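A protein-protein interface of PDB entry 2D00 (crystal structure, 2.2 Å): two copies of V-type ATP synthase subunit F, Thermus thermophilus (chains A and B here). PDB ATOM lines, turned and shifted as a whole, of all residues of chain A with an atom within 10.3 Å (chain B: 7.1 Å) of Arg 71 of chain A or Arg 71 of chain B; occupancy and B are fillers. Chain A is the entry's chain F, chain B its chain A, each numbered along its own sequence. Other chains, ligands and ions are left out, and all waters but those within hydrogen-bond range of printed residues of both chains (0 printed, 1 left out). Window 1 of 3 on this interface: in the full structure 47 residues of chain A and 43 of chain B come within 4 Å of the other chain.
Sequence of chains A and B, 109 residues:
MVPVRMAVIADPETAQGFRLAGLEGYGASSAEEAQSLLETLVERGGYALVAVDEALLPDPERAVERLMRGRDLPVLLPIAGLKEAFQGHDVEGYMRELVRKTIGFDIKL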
ATOM      1  N   GLN A  35     -25.808  10.810  24.905  1.00  0.00           N
ATOM      2  CA  GLN A  35     -25.828  11.600  23.707  1.00  0.00           C
ATOM      3  C   GLN A  35     -25.887  10.731  22.367  1.00  0.00           C
ATOM      4  O   GLN A  35     -26.462  11.145  21.388  1.00  0.00           O
ATOM      5  CB  GLN A  35     -24.591  12.472  23.681  1.00  0.00           C
ATOM      6  CG  GLN A  35     -24.567  13.568  22.462  1.00  0.00           C
ATOM      7  CD  GLN A  35     -25.508  14.711  22.697  1.00  0.00           C
ATOM      8  OE1 GLN A  35     -25.763  14.968  23.851  1.00  0.00           O
ATOM      9  NE2 GLN A  35     -26.057  15.405  21.610  1.00  0.00           N
ATOM     10  N   SER A  36     -25.182   9.606  22.313  1.00  0.00           N
ATOM     11  CA  SER A  36     -25.334   8.672  21.134  1.00  0.00           C
ATOM     12  C   SER A  36     -26.800   8.271  20.932  1.00  0.00           C
ATOM     13  O   SER A  36     -27.269   8.185  19.838  1.00  0.00           O
ATOM     14  CB  SER A  36     -24.562   7.418  21.360  1.00  0.00           C
ATOM     15  OG  SER A  36     -24.587   6.462  20.292  1.00  0.00           O
ATOM     16  N   LEU A  37     -27.467   7.909  21.993  1.00  0.00           N
ATOM     17  CA  LEU A  37     -28.809   7.390  21.916  1.00  0.00           C
ATOM     18  C   LEU A  37     -29.689   8.494  21.477  1.00  0.00           C
ATOM     19  O   LEU A  37     -30.557   8.280  20.679  1.00  0.00           O
ATOM     20  CB  LEU A  37     -29.257   6.930  23.279  1.00  0.00           C
ATOM     21  CG  LEU A  37     -28.678   5.550  23.656  1.00  0.00           C
ATOM     22  CD1 LEU A  37     -28.929   5.360  25.073  1.00  0.00           C
ATOM     23  CD2 LEU A  37     -29.321   4.425  22.867  1.00  0.00           C
ATOM     24  N   LEU A  38     -29.447   9.733  21.916  1.00  0.00           N
ATOM     25  CA  LEU A  38     -30.309  10.848  21.467  1.00  0.00           C
ATOM     26  C   LEU A  38     -30.179  11.033  20.017  1.00  0.00           C
ATOM     27  O   LEU A  38     -31.153  11.369  19.339  1.00  0.00           O
ATOM     28  CB  LEU A  38     -29.903  12.153  22.180  1.00  0.00           C
ATOM     29  CG  LEU A  38     -30.314  12.310  23.602  1.00  0.00           C
ATOM     30  CD1 LEU A  38     -29.771  13.629  24.213  1.00  0.00           C
ATOM     31  CD2 LEU A  38     -31.844  12.292  23.643  1.00  0.00           C
ATOM     32  N   GLU A  39     -28.935  10.944  19.510  1.00  0.00           N
ATOM     33  CA  GLU A  39     -28.680  11.072  18.050  1.00  0.00           C
ATOM     34  C   GLU A  39     -29.381  10.003  17.276  1.00  0.00           C
ATOM     35  O   GLU A  39     -30.010  10.243  16.190  1.00  0.00           O
ATOM     36  CB  GLU A  39     -27.182  11.179  17.789  1.00  0.00           C
ATOM     37  CG  GLU A  39     -26.720  11.174  16.463  1.00  0.00           C
ATOM     38  CD  GLU A  39     -27.181  12.403  15.655  1.00  0.00           C
ATOM     39  OE1 GLU A  39     -27.198  13.486  16.239  1.00  0.00           O
ATOM     40  OE2 GLU A  39     -27.481  12.261  14.451  1.00  0.00           O
ATOM     41  N   THR A  40     -29.313   8.782  17.808  1.00  0.00           N
ATOM     42  CA  THR A  40     -30.000   7.633  17.141  1.00  0.00           C
ATOM     43  C   THR A  40     -31.585   7.889  17.069  1.00  0.00           C
ATOM     44  O   THR A  40     -32.198   7.640  16.071  1.00  0.00           O
ATOM     45  CB  THR A  40     -29.772   6.322  18.006  1.00  0.00           C
ATOM     46  OG1 THR A  40     -28.446   5.871  17.851  1.00  0.00           O
ATOM     47  CG2 THR A  40     -30.723   5.158  17.610  1.00  0.00           C
ATOM     48  N   LEU A  41     -32.182   8.375  18.171  1.00  0.00           N
ATOM     49  CA  LEU A  41     -33.619   8.677  18.227  1.00  0.00           C
ATOM     50  C   LEU A  41     -33.957   9.815  17.362  1.00  0.00           C
ATOM     51  O   LEU A  41     -34.979   9.804  16.682  1.00  0.00           O
ATOM     52  CB  LEU A  41     -34.029   9.033  19.659  1.00  0.00           C
ATOM     53  CG  LEU A  41     -33.901   7.870  20.622  1.00  0.00           C
ATOM     54  CD1 LEU A  41     -34.086   8.297  22.054  1.00  0.00           C
ATOM     55  CD2 LEU A  41     -34.691   6.678  20.227  1.00  0.00           C
ATOM     56  N   VAL A  42     -33.092  10.827  17.357  1.00  0.00           N
ATOM     57  CA  VAL A  42     -33.356  12.018  16.485  1.00  0.00           C
ATOM     58  C   VAL A  42     -33.407  11.578  15.053  1.00  0.00           C
ATOM     59  O   VAL A  42     -34.324  11.964  14.254  1.00  0.00           O
ATOM     60  CB  VAL A  42     -32.421  13.261  16.716  1.00  0.00           C
ATOM     61  CG1 VAL A  42     -32.538  14.220  15.629  1.00  0.00           C
ATOM     62  CG2 VAL A  42     -32.820  13.964  17.966  1.00  0.00           C
ATOM     63  N   GLU A  43     -32.417  10.800  14.724  1.00  0.00           N
ATOM     64  CA  GLU A  43     -32.253  10.237  13.357  1.00  0.00           C
ATOM     65  C   GLU A  43     -33.419   9.275  12.980  1.00  0.00           C
ATOM     66  O   GLU A  43     -33.884   9.296  11.856  1.00  0.00           O
ATOM     67  CB  GLU A  43     -30.870   9.525  13.292  1.00  0.00           C
ATOM     68  CG  GLU A  43     -30.366   9.147  12.004  1.00  0.00           C
ATOM     69  CD  GLU A  43     -30.638  10.252  10.972  1.00  0.00           C
ATOM     70  OE1 GLU A  43     -30.445  11.463  11.359  1.00  0.00           O
ATOM     71  OE2 GLU A  43     -31.113   9.901   9.865  1.00  0.00           O
ATOM     72  N   ARG A  44     -33.923   8.440  13.894  1.00  0.00           N
ATOM     73  CA  ARG A  44     -35.177   7.682  13.525  1.00  0.00           C
ATOM     74  C   ARG A  44     -36.346   8.593  13.148  1.00  0.00           C
ATOM     75  O   ARG A  44     -37.019   8.399  12.174  1.00  0.00           O
ATOM     76  CB  ARG A  44     -35.620   6.823  14.661  1.00  0.00           C
ATOM     77  CG  ARG A  44     -34.948   5.492  14.519  1.00  0.00           C
ATOM     78  CD  ARG A  44     -34.409   4.931  15.801  1.00  0.00           C
ATOM     79  NE  ARG A  44     -35.395   4.323  16.672  1.00  0.00           N
ATOM     80  CZ  ARG A  44     -35.069   3.559  17.736  1.00  0.00           C
ATOM     81  NH1 ARG A  44     -33.799   3.267  18.046  1.00  0.00           N
ATOM     82  NH2 ARG A  44     -36.004   3.071  18.519  1.00  0.00           N
ATOM     83  N   GLY A  45     -36.586   9.591  13.974  1.00  0.00           N
ATOM     84  CA  GLY A  45     -37.487  10.714  13.652  1.00  0.00           C
ATOM     85  C   GLY A  45     -38.845  10.687  14.370  1.00  0.00           C
ATOM     86  O   GLY A  45     -39.653  11.642  14.236  1.00  0.00           O
ATOM     87  N   ALA A  63     -26.289  19.645  24.719  1.00  0.00           N
ATOM     88  CA  ALA A  63     -26.805  18.475  24.138  1.00  0.00           C
ATOM     89  C   ALA A  63     -27.604  18.786  22.802  1.00  0.00           C
ATOM     90  O   ALA A  63     -27.490  18.100  21.807  1.00  0.00           O
ATOM     91  CB  ALA A  63     -27.731  17.761  25.065  1.00  0.00           C
ATOM     92  N   VAL A  64     -28.448  19.783  22.894  1.00  0.00           N
ATOM     93  CA  VAL A  64     -29.227  20.299  21.782  1.00  0.00           C
ATOM     94  C   VAL A  64     -28.281  20.890  20.708  1.00  0.00           C
ATOM     95  O   VAL A  64     -28.513  20.712  19.478  1.00  0.00           O
ATOM     96  CB  VAL A  64     -30.242  21.373  22.345  1.00  0.00           C
ATOM     97  CG1 VAL A  64     -30.951  22.064  21.257  1.00  0.00           C
ATOM     98  CG2 VAL A  64     -31.181  20.738  23.337  1.00  0.00           C
ATOM     99  N   GLU A  65     -27.245  21.635  21.137  1.00  0.00           N
ATOM    100  CA  GLU A  65     -26.385  22.230  20.196  1.00  0.00           C
ATOM    101  C   GLU A  65     -25.671  21.100  19.418  1.00  0.00           C
ATOM    102  O   GLU A  65     -25.567  21.142  18.205  1.00  0.00           O
ATOM    103  CB  GLU A  65     -25.432  23.168  20.888  1.00  0.00           C
ATOM    104  CG  GLU A  65     -24.502  23.951  20.026  1.00  0.00           C
ATOM    105  CD  GLU A  65     -23.084  23.861  20.558  1.00  0.00           C
ATOM    106  OE1 GLU A  65     -22.766  24.549  21.580  1.00  0.00           O
ATOM    107  OE2 GLU A  65     -22.304  23.057  19.946  1.00  0.00           O
ATOM    108  N   ARG A  66     -25.245  20.048  20.096  1.00  0.00           N
ATOM    109  CA  ARG A  66     -24.682  18.907  19.353  1.00  0.00           C
ATOM    110  C   ARG A  66     -25.671  18.188  18.347  1.00  0.00           C
ATOM    111  O   ARG A  66     -25.330  17.947  17.199  1.00  0.00           O
ATOM    112  CB  ARG A  66     -23.999  17.948  20.277  1.00  0.00           C
ATOM    113  CG  ARG A  66     -22.715  18.640  20.921  1.00  0.00           C
ATOM    114  CD  ARG A  66     -22.151  17.758  21.942  1.00  0.00           C
ATOM    115  NE  ARG A  66     -21.771  16.494  21.298  1.00  0.00           N
ATOM    116  CZ  ARG A  66     -21.255  15.430  21.918  1.00  0.00           C
ATOM    117  NH1 ARG A  66     -21.102  15.443  23.253  1.00  0.00           N
ATOM    118  NH2 ARG A  66     -20.968  14.346  21.172  1.00  0.00           N
ATOM    119  N   LEU A  67     -26.906  18.000  18.770  1.00  0.00           N
ATOM    120  CA  LEU A  67     -28.017  17.530  17.880  1.00  0.00           C
ATOM    121  C   LEU A  67     -28.217  18.368  16.596  1.00  0.00           C
ATOM    122  O   LEU A  67     -28.223  17.842  15.515  1.00  0.00           O
ATOM    123  CB  LEU A  67     -29.322  17.379  18.679  1.00  0.00           C
ATOM    124  CG  LEU A  67     -29.268  16.248  19.675  1.00  0.00           C
ATOM    125  CD1 LEU A  67     -30.585  16.158  20.486  1.00  0.00           C
ATOM    126  CD2 LEU A  67     -28.943  14.865  19.092  1.00  0.00           C
ATOM    127  N   MET A  68     -28.221  19.676  16.704  1.00  0.00           N
ATOM    128  CA  MET A  68     -28.448  20.529  15.552  1.00  0.00           C
ATOM    129  C   MET A  68     -27.256  20.652  14.678  1.00  0.00           C
ATOM    130  O   MET A  68     -27.331  20.619  13.453  1.00  0.00           O
ATOM    131  CB  MET A  68     -28.730  21.937  16.030  1.00  0.00           C
ATOM    132  CG  MET A  68     -29.771  22.027  17.055  1.00  0.00           C
ATOM    133  SD  MET A  68     -31.400  21.715  16.451  1.00  0.00           S
ATOM    134  CE  MET A  68     -31.352  20.272  15.492  1.00  0.00           C
ATOM    135  N   ARG A  69     -26.154  20.722  15.347  1.00  0.00           N
ATOM    136  CA  ARG A  69     -25.015  21.496  14.936  1.00  0.00           C
ATOM    137  C   ARG A  69     -23.833  20.545  14.922  1.00  0.00           C
ATOM    138  O   ARG A  69     -22.708  21.014  15.164  1.00  0.00           O
ATOM    139  CB  ARG A  69     -24.787  22.652  16.001  1.00  0.00           C
ATOM    140  CG  ARG A  69     -24.023  23.904  15.618  1.00  0.00           C
ATOM    141  CD  ARG A  69     -22.825  24.258  16.565  1.00  0.00           C
ATOM    142  NE  ARG A  69     -21.877  25.187  15.867  1.00  0.00           N
ATOM    143  CZ  ARG A  69     -20.809  25.791  16.428  1.00  0.00           C
ATOM    144  NH1 ARG A  69     -20.499  25.596  17.716  1.00  0.00           N
ATOM    145  NH2 ARG A  69     -20.046  26.610  15.703  1.00  0.00           N
ATOM    146  N   GLY A  70     -24.002  19.282  14.547  1.00  0.00           N
ATOM    147  CA  GLY A  70     -22.891  18.323  14.727  1.00  0.00           C
ATOM    148  C   GLY A  70     -22.781  17.143  13.776  1.00  0.00           C
ATOM    149  O   GLY A  70     -21.690  16.554  13.616  1.00  0.00           O
ATOM    150  N   ARG A  71     -23.908  16.760  13.188  1.00  0.00           N
ATOM    151  CA  ARG A  71     -23.908  15.693  12.235  1.00  0.00           C
ATOM    152  C   ARG A  71     -22.969  16.072  11.005  1.00  0.00           C
ATOM    153  O   ARG A  71     -22.743  17.276  10.698  1.00  0.00           O
ATOM    154  CB  ARG A  71     -25.380  15.371  11.863  1.00  0.00           C
ATOM    155  CG  ARG A  71     -25.844  16.040  10.509  1.00  0.00           C
ATOM    156  CD  ARG A  71     -27.347  15.975  10.399  1.00  0.00           C
ATOM    157  NE  ARG A  71     -27.958  17.296  10.204  1.00  0.00           N
ATOM    158  CZ  ARG A  71     -29.180  17.476   9.735  1.00  0.00           C
ATOM    159  NH1 ARG A  71     -29.942  16.437   9.407  1.00  0.00           N
ATOM    160  NH2 ARG A  71     -29.642  18.699   9.612  1.00  0.00           N
ATOM    161  N   ASP A  72     -22.448  15.036  10.319  1.00  0.00           N
ATOM    162  CA  ASP A  72     -21.341  15.134   9.341  1.00  0.00           C
ATOM    163  C   ASP A  72     -21.812  15.679   7.990  1.00  0.00           C
ATOM    164  O   ASP A  72     -22.666  15.071   7.360  1.00  0.00           O
ATOM    165  CB  ASP A  72     -20.673  13.744   9.142  1.00  0.00           C
ATOM    166  CG  ASP A  72     -19.667  13.365  10.301  1.00  0.00           C
ATOM    167  OD1 ASP A  72     -19.041  14.285  10.935  1.00  0.00           O
ATOM    168  OD2 ASP A  72     -19.481  12.139  10.548  1.00  0.00           O
ATOM    169  N   LEU A  73     -21.248  16.800   7.554  1.00  0.00           N
ATOM    170  CA  LEU A  73     -21.766  17.513   6.371  1.00  0.00           C
ATOM    171  C   LEU A  73     -21.087  17.099   5.051  1.00  0.00           C
ATOM    172  O   LEU A  73     -19.892  16.725   5.053  1.00  0.00           O
ATOM    173  CB  LEU A  73     -21.701  19.075   6.548  1.00  0.00           C
ATOM    174  CG  LEU A  73     -22.534  19.783   7.662  1.00  0.00           C
ATOM    175  CD1 LEU A  73     -22.395  21.350   7.663  1.00  0.00           C
ATOM    176  CD2 LEU A  73     -24.028  19.458   7.564  1.00  0.00           C
ATOM    177  N   PRO A  74     -21.878  17.127   3.937  1.00  0.00           N
ATOM    178  CA  PRO A  74     -21.505  17.257   2.478  1.00  0.00           C
ATOM    179  C   PRO A  74     -20.567  18.450   2.288  1.00  0.00           C
ATOM    180  O   PRO A  74     -20.910  19.486   2.827  1.00  0.00           O
ATOM    181  CB  PRO A  74     -22.808  17.625   1.845  1.00  0.00           C
ATOM    182  CG  PRO A  74     -23.877  17.080   2.808  1.00  0.00           C
ATOM    183  CD  PRO A  74     -23.339  16.966   4.121  1.00  0.00           C
ATOM    184  N   VAL A  75     -19.393  18.354   1.650  1.00  0.00           N
ATOM    185  CA  VAL A  75     -18.681  19.564   1.232  1.00  0.00           C
ATOM    186  C   VAL A  75     -19.665  20.362   0.331  1.00  0.00           C
ATOM    187  O   VAL A  75     -20.584  19.794  -0.277  1.00  0.00           O
ATOM    188  CB  VAL A  75     -17.375  19.216   0.526  1.00  0.00           C
ATOM    189  CG1 VAL A  75     -16.664  20.438  -0.014  1.00  0.00           C
ATOM    190  CG2 VAL A  75     -16.411  18.437   1.501  1.00  0.00           C
ATOM    191  N   GLU B  39     -30.952  21.445   2.513  1.00  0.00           N
ATOM    192  CA  GLU B  39     -31.461  20.851   3.735  1.00  0.00           C
ATOM    193  C   GLU B  39     -32.125  19.508   3.426  1.00  0.00           C
ATOM    194  O   GLU B  39     -31.642  18.420   4.217  1.00  0.00           O
ATOM    195  CB  GLU B  39     -32.341  21.820   4.537  1.00  0.00           C
ATOM    196  CG  GLU B  39     -33.023  21.246   5.854  1.00  0.00           C
ATOM    197  CD  GLU B  39     -32.628  22.011   7.092  1.00  0.00           C
ATOM    198  OE1 GLU B  39     -32.439  23.294   6.936  1.00  0.00           O
ATOM    199  OE2 GLU B  39     -32.506  21.361   8.198  1.00  0.00           O
ATOM    200  N   VAL B  42     -29.424  17.157   2.831  1.00  0.00           N
ATOM    201  CA  VAL B  42     -28.623  16.870   4.054  1.00  0.00           C
ATOM    202  C   VAL B  42     -29.284  15.871   5.005  1.00  0.00           C
ATOM    203  O   VAL B  42     -28.599  14.971   5.481  1.00  0.00           O
ATOM    204  CB  VAL B  42     -28.211  18.193   4.744  1.00  0.00           C
ATOM    205  CG1 VAL B  42     -27.724  17.983   6.201  1.00  0.00           C
ATOM    206  CG2 VAL B  42     -27.119  18.864   3.884  1.00  0.00           C
ATOM    207  N   GLU B  43     -30.608  16.000   5.158  1.00  0.00           N
ATOM    208  CA  GLU B  43     -31.394  15.226   6.077  1.00  0.00           C
ATOM    209  C   GLU B  43     -31.486  13.863   5.471  1.00  0.00           C
ATOM    210  O   GLU B  43     -31.514  12.850   6.204  1.00  0.00           O
ATOM    211  CB  GLU B  43     -32.888  15.736   6.228  1.00  0.00           C
ATOM    212  CG  GLU B  43     -33.082  17.299   6.456  1.00  0.00           C
ATOM    213  CD  GLU B  43     -32.776  17.713   8.087  1.00  0.00           C
ATOM    214  OE1 GLU B  43     -33.287  16.880   8.986  1.00  0.00           O
ATOM    215  OE2 GLU B  43     -32.069  18.791   8.295  1.00  0.00           O
ATOM    216  N   ARG B  44     -31.514  13.869   4.065  1.00  0.00           N
ATOM    217  CA  ARG B  44     -31.861  12.595   3.445  1.00  0.00           C
ATOM    218  C   ARG B  44     -30.627  11.668   3.436  1.00  0.00           C
ATOM    219  O   ARG B  44     -30.757  10.437   3.581  1.00  0.00           O
ATOM    220  CB  ARG B  44     -32.417  12.795   2.067  1.00  0.00           C
ATOM    221  CG  ARG B  44     -32.858  11.447   1.514  1.00  0.00           C
ATOM    222  CD  ARG B  44     -33.508  11.631   0.228  1.00  0.00           C
ATOM    223  NE  ARG B  44     -32.623  12.303  -0.701  1.00  0.00           N
ATOM    224  CZ  ARG B  44     -32.916  12.462  -1.981  1.00  0.00           C
ATOM    225  NH1 ARG B  44     -34.047  11.965  -2.487  1.00  0.00           N
ATOM    226  NH2 ARG B  44     -32.076  13.079  -2.762  1.00  0.00           N
ATOM    227  N   ARG B  66     -27.212  27.579   8.355  1.00  0.00           N
ATOM    228  CA  ARG B  66     -28.652  27.283   8.466  1.00  0.00           C
ATOM    229  C   ARG B  66     -29.032  25.775   8.450  1.00  0.00           C
ATOM    230  O   ARG B  66     -30.045  25.410   9.039  1.00  0.00           O
ATOM    231  CB  ARG B  66     -29.422  27.967   7.350  1.00  0.00           C
ATOM    232  CG  ARG B  66     -28.996  29.398   7.121  1.00  0.00           C
ATOM    233  CD  ARG B  66     -29.551  29.897   5.871  1.00  0.00           C
ATOM    234  NE  ARG B  66     -31.002  29.911   5.962  1.00  0.00           N
ATOM    235  CZ  ARG B  66     -31.741  30.504   5.045  1.00  0.00           C
ATOM    236  NH1 ARG B  66     -31.132  31.080   4.011  1.00  0.00           N
ATOM    237  NH2 ARG B  66     -33.067  30.512   5.149  1.00  0.00           N
ATOM    238  N   LEU B  67     -28.278  24.957   7.675  1.00  0.00           N
ATOM    239  CA  LEU B  67     -28.597  23.565   7.477  1.00  0.00           C
ATOM    240  C   LEU B  67     -28.713  22.889   8.813  1.00  0.00           C
ATOM    241  O   LEU B  67     -29.544  21.977   9.050  1.00  0.00           O
ATOM    242  CB  LEU B  67     -27.454  22.882   6.738  1.00  0.00           C
ATOM    243  CG  LEU B  67     -27.501  23.103   5.214  1.00  0.00           C
ATOM    244  CD1 LEU B  67     -26.313  22.439   4.455  1.00  0.00           C
ATOM    245  CD2 LEU B  67     -28.869  22.567   4.753  1.00  0.00           C
ATOM    246  N   MET B  68     -27.812  23.314   9.671  1.00  0.00           N
ATOM    247  CA  MET B  68     -27.715  22.756  10.949  1.00  0.00           C
ATOM    248  C   MET B  68     -28.634  23.437  11.977  1.00  0.00           C
ATOM    249  O   MET B  68     -28.429  23.224  13.176  1.00  0.00           O
ATOM    250  CB  MET B  68     -26.232  22.691  11.367  1.00  0.00           C
ATOM    251  CG  MET B  68     -25.496  23.993  11.680  1.00  0.00           C
ATOM    252  SD  MET B  68     -23.736  23.643  11.394  1.00  0.00           S
ATOM    253  CE  MET B  68     -23.186  25.268  10.807  1.00  0.00           C
ATOM    254  N   ARG B  69     -29.661  24.178  11.522  1.00  0.00           N
ATOM    255  CA  ARG B  69     -30.711  24.671  12.418  1.00  0.00           C
ATOM    256  C   ARG B  69     -32.159  24.377  11.947  1.00  0.00           C
ATOM    257  O   ARG B  69     -33.169  24.920  12.534  1.00  0.00           O
ATOM    258  CB  ARG B  69     -30.512  26.155  12.708  1.00  0.00           C
ATOM    259  CG  ARG B  69     -29.137  26.611  12.308  1.00  0.00           C
ATOM    260  CD  ARG B  69     -28.682  27.804  13.019  1.00  0.00           C
ATOM    261  NE  ARG B  69     -27.837  27.402  14.143  1.00  0.00           N
ATOM    262  CZ  ARG B  69     -26.844  28.149  14.622  1.00  0.00           C
ATOM    263  NH1 ARG B  69     -26.558  29.349  14.063  1.00  0.00           N
ATOM    264  NH2 ARG B  69     -26.122  27.695  15.646  1.00  0.00           N
ATOM    265  N   GLY B  70     -32.246  23.467  10.938  1.00  0.00           N
ATOM    266  CA  GLY B  70     -33.521  22.984  10.426  1.00  0.00           C
ATOM    267  C   GLY B  70     -33.917  21.581  10.915  1.00  0.00           C
ATOM    268  O   GLY B  70     -34.968  21.071  10.544  1.00  0.00           O
ATOM    269  N   ARG B  71     -33.064  20.917  11.677  1.00  0.00           N
ATOM    270  CA  ARG B  71     -33.338  19.564  12.167  1.00  0.00           C
ATOM    271  C   ARG B  71     -34.434  19.708  13.238  1.00  0.00           C
ATOM    272  O   ARG B  71     -34.307  20.547  14.087  1.00  0.00           O
ATOM    273  CB  ARG B  71     -32.105  18.936  12.837  1.00  0.00           C
ATOM    274  CG  ARG B  71     -32.004  17.407  12.727  1.00  0.00           C
ATOM    275  CD  ARG B  71     -30.785  16.934  13.540  1.00  0.00           C
ATOM    276  NE  ARG B  71     -30.529  15.584  13.196  1.00  0.00           N
ATOM    277  CZ  ARG B  71     -29.689  14.761  13.773  1.00  0.00           C
ATOM    278  NH1 ARG B  71     -28.875  15.145  14.766  1.00  0.00           N
ATOM    279  NH2 ARG B  71     -29.597  13.533  13.256  1.00  0.00           N
ATOM    280  N   ASP B  72     -35.476  18.900  13.126  1.00  0.00           N
ATOM    281  CA  ASP B  72     -36.593  18.804  14.063  1.00  0.00           C
ATOM    282  C   ASP B  72     -36.154  17.987  15.209  1.00  0.00           C
ATOM    283  O   ASP B  72     -35.680  16.934  15.046  1.00  0.00           O
ATOM    284  CB  ASP B  72     -37.834  18.075  13.468  1.00  0.00           C
ATOM    285  CG  ASP B  72     -38.786  19.029  12.719  1.00  0.00           C
ATOM    286  OD1 ASP B  72     -38.269  20.090  12.486  1.00  0.00           O
ATOM    287  OD2 ASP B  72     -39.972  18.777  12.328  1.00  0.00           O
ATOM    288  N   LEU B  73     -36.285  18.503  16.413  1.00  0.00           N
ATOM    289  CA  LEU B  73     -35.883  17.690  17.516  1.00  0.00           C
ATOM    290  C   LEU B  73     -37.066  17.309  18.423  1.00  0.00           C
ATOM    291  O   LEU B  73     -37.956  18.058  18.610  1.00  0.00           O
ATOM    292  CB  LEU B  73     -34.835  18.474  18.366  1.00  0.00           C
ATOM    293  CG  LEU B  73     -33.517  18.957  17.735  1.00  0.00           C
ATOM    294  CD1 LEU B  73     -32.617  19.278  18.823  1.00  0.00           C
ATOM    295  CD2 LEU B  73     -32.917  17.852  16.938  1.00  0.00           C
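The side-chain carboxylate of Glu 43 of chain B lies within salt-bridge range of the guanidinium group of Arg 71 of chain A.
The backbone carbonyl oxygen (O) of Leu 67 of chain B lies within hydrogen-bond range of the guanidinium group (NH2) of Arg 71 of chain A (3.3 Å).
NH2 of Arg 71 of chain B lies within salt-bridge range of OE2 of Glu 39 of chain A, 2.7 Å away.
NH2 of Arg 71 of chain B lies within salt-bridge range of OE1 of Glu 43 of chain A, at 2.9 Å.
NH1 of Arg 71 of chain B sits at hydrogen-bond distance from O of Leu 67 of chain A, at 2.9 Å.
The backbone carbonyl oxygen of Met 68 of chain A lies close to the backbone carbonyl oxygen of Met 68 of chain B, 2.8 Å away.
The side-chain carboxylate (OE2) of Glu 43 of chain B lies close to the side-chain carboxylate (OE2) of Glu 39 of chain B (2.6 Å).
The guanidinium group (NH1) of Arg 69 of chain A lies within salt-bridge range of the side-chain carboxylate (OE2) of Glu 65 of chain A (3.8 Å).
Arg 71 of chain B touches Val 42 of chain A (NE to CG1, 3.4 Å).
CG1 of Val 42 of chain A touches CD2 of Leu 73 of chain B (3.9 Å).
Leu 73 of chain B touches Leu 67 of chain A.
Met 68 of chain A touches Arg 71 of chain B.
Met 68 of chain A touches Leu 73 of chain B (CE to CD2, 3.2 Å).
Met 68 of chain B touches Arg 69 of chain A (CB to CA, 3.96 Å).
Arg 71 of chain A touches Val 42 of chain B.
NH1 of Arg 71 of chain A touches NE of Arg 71 of chain B, at 3.9 Å.
CG of Pro 74 of chain A touches CG2 of Val 42 of chain B, 3.9 Å away.
Printed residues of chain B within 4 Å of Glu 39 of chain A: Arg 71.
Of the printed residues of chain B, Glu 43 of chain A touches Arg 71 (2.9 Å).
Ala 63 of chain A touches none of the printed residues of chain B.
Of the printed residues of chain B, Met 68 of chain A touches Met 68, Arg 71 and Leu 73.
Printed residues of chain B within 4 Å of Arg 69 of chain A: Met 68.
No residue of chain B comes within 4 Å of Gly 70 of chain A.
Arg 71 of chain A touches just these residues of chain B: Val 42 (3.9 Å), Glu 43 (2.8 Å), Leu 67 (3.3 Å) and Arg 71 (3.9 Å).
Printed residues of chain A within 4 Å of Val 42 of chain B: Arg 71 (3.9 Å) and Pro 74 (3.9 Å).
The nearest residue of chain B that does not touch Arg 71 of chain A is Glu 39 of chain B (4.2 Å).
Hydrophobic or aromatic side chains of chain B within 4 Å of the printed part of chain A: Val 42, Met 68 and Leu 73.
Of the 24 printed residues of chain A, 8 touch a printed residue of chain B.
Among the printed residues, Asp or Glu carboxylates within 4 Å of a Lys or Arg side-chain nitrogen of the other chain: Glu 39 of chain A with Arg 71 of chain B (2.7 Å), Glu 43 of chain A with Arg 71 of chain B (2.9 Å) and Arg 71 of chain A with Glu 43 of chain B (2.8 Å).
Val 42 of chain A touches Arg 71 of chain B, and with the chains exchanged Arg 71 of chain A touches Val 42 of chain B.
Met 68 of chain A touches its own counterpart, Met 68 of chain B.
Met 68 of chain A touches Arg 71 of chain B, but with the chains exchanged Arg 71 of chain A does not touch Met 68 of chain B (4.7 Å).
Arg 71 of chain A touches its own counterpart, Arg 71 of chain B.
Positions printed for both chains: 39, 42, 43, 44, 66, 67, 68, 69, 70, 71, 72 and 73.
Of the 15 pairs that touch across the chains among the printed residues, 8 have their exchanged pair printed and touching as well.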
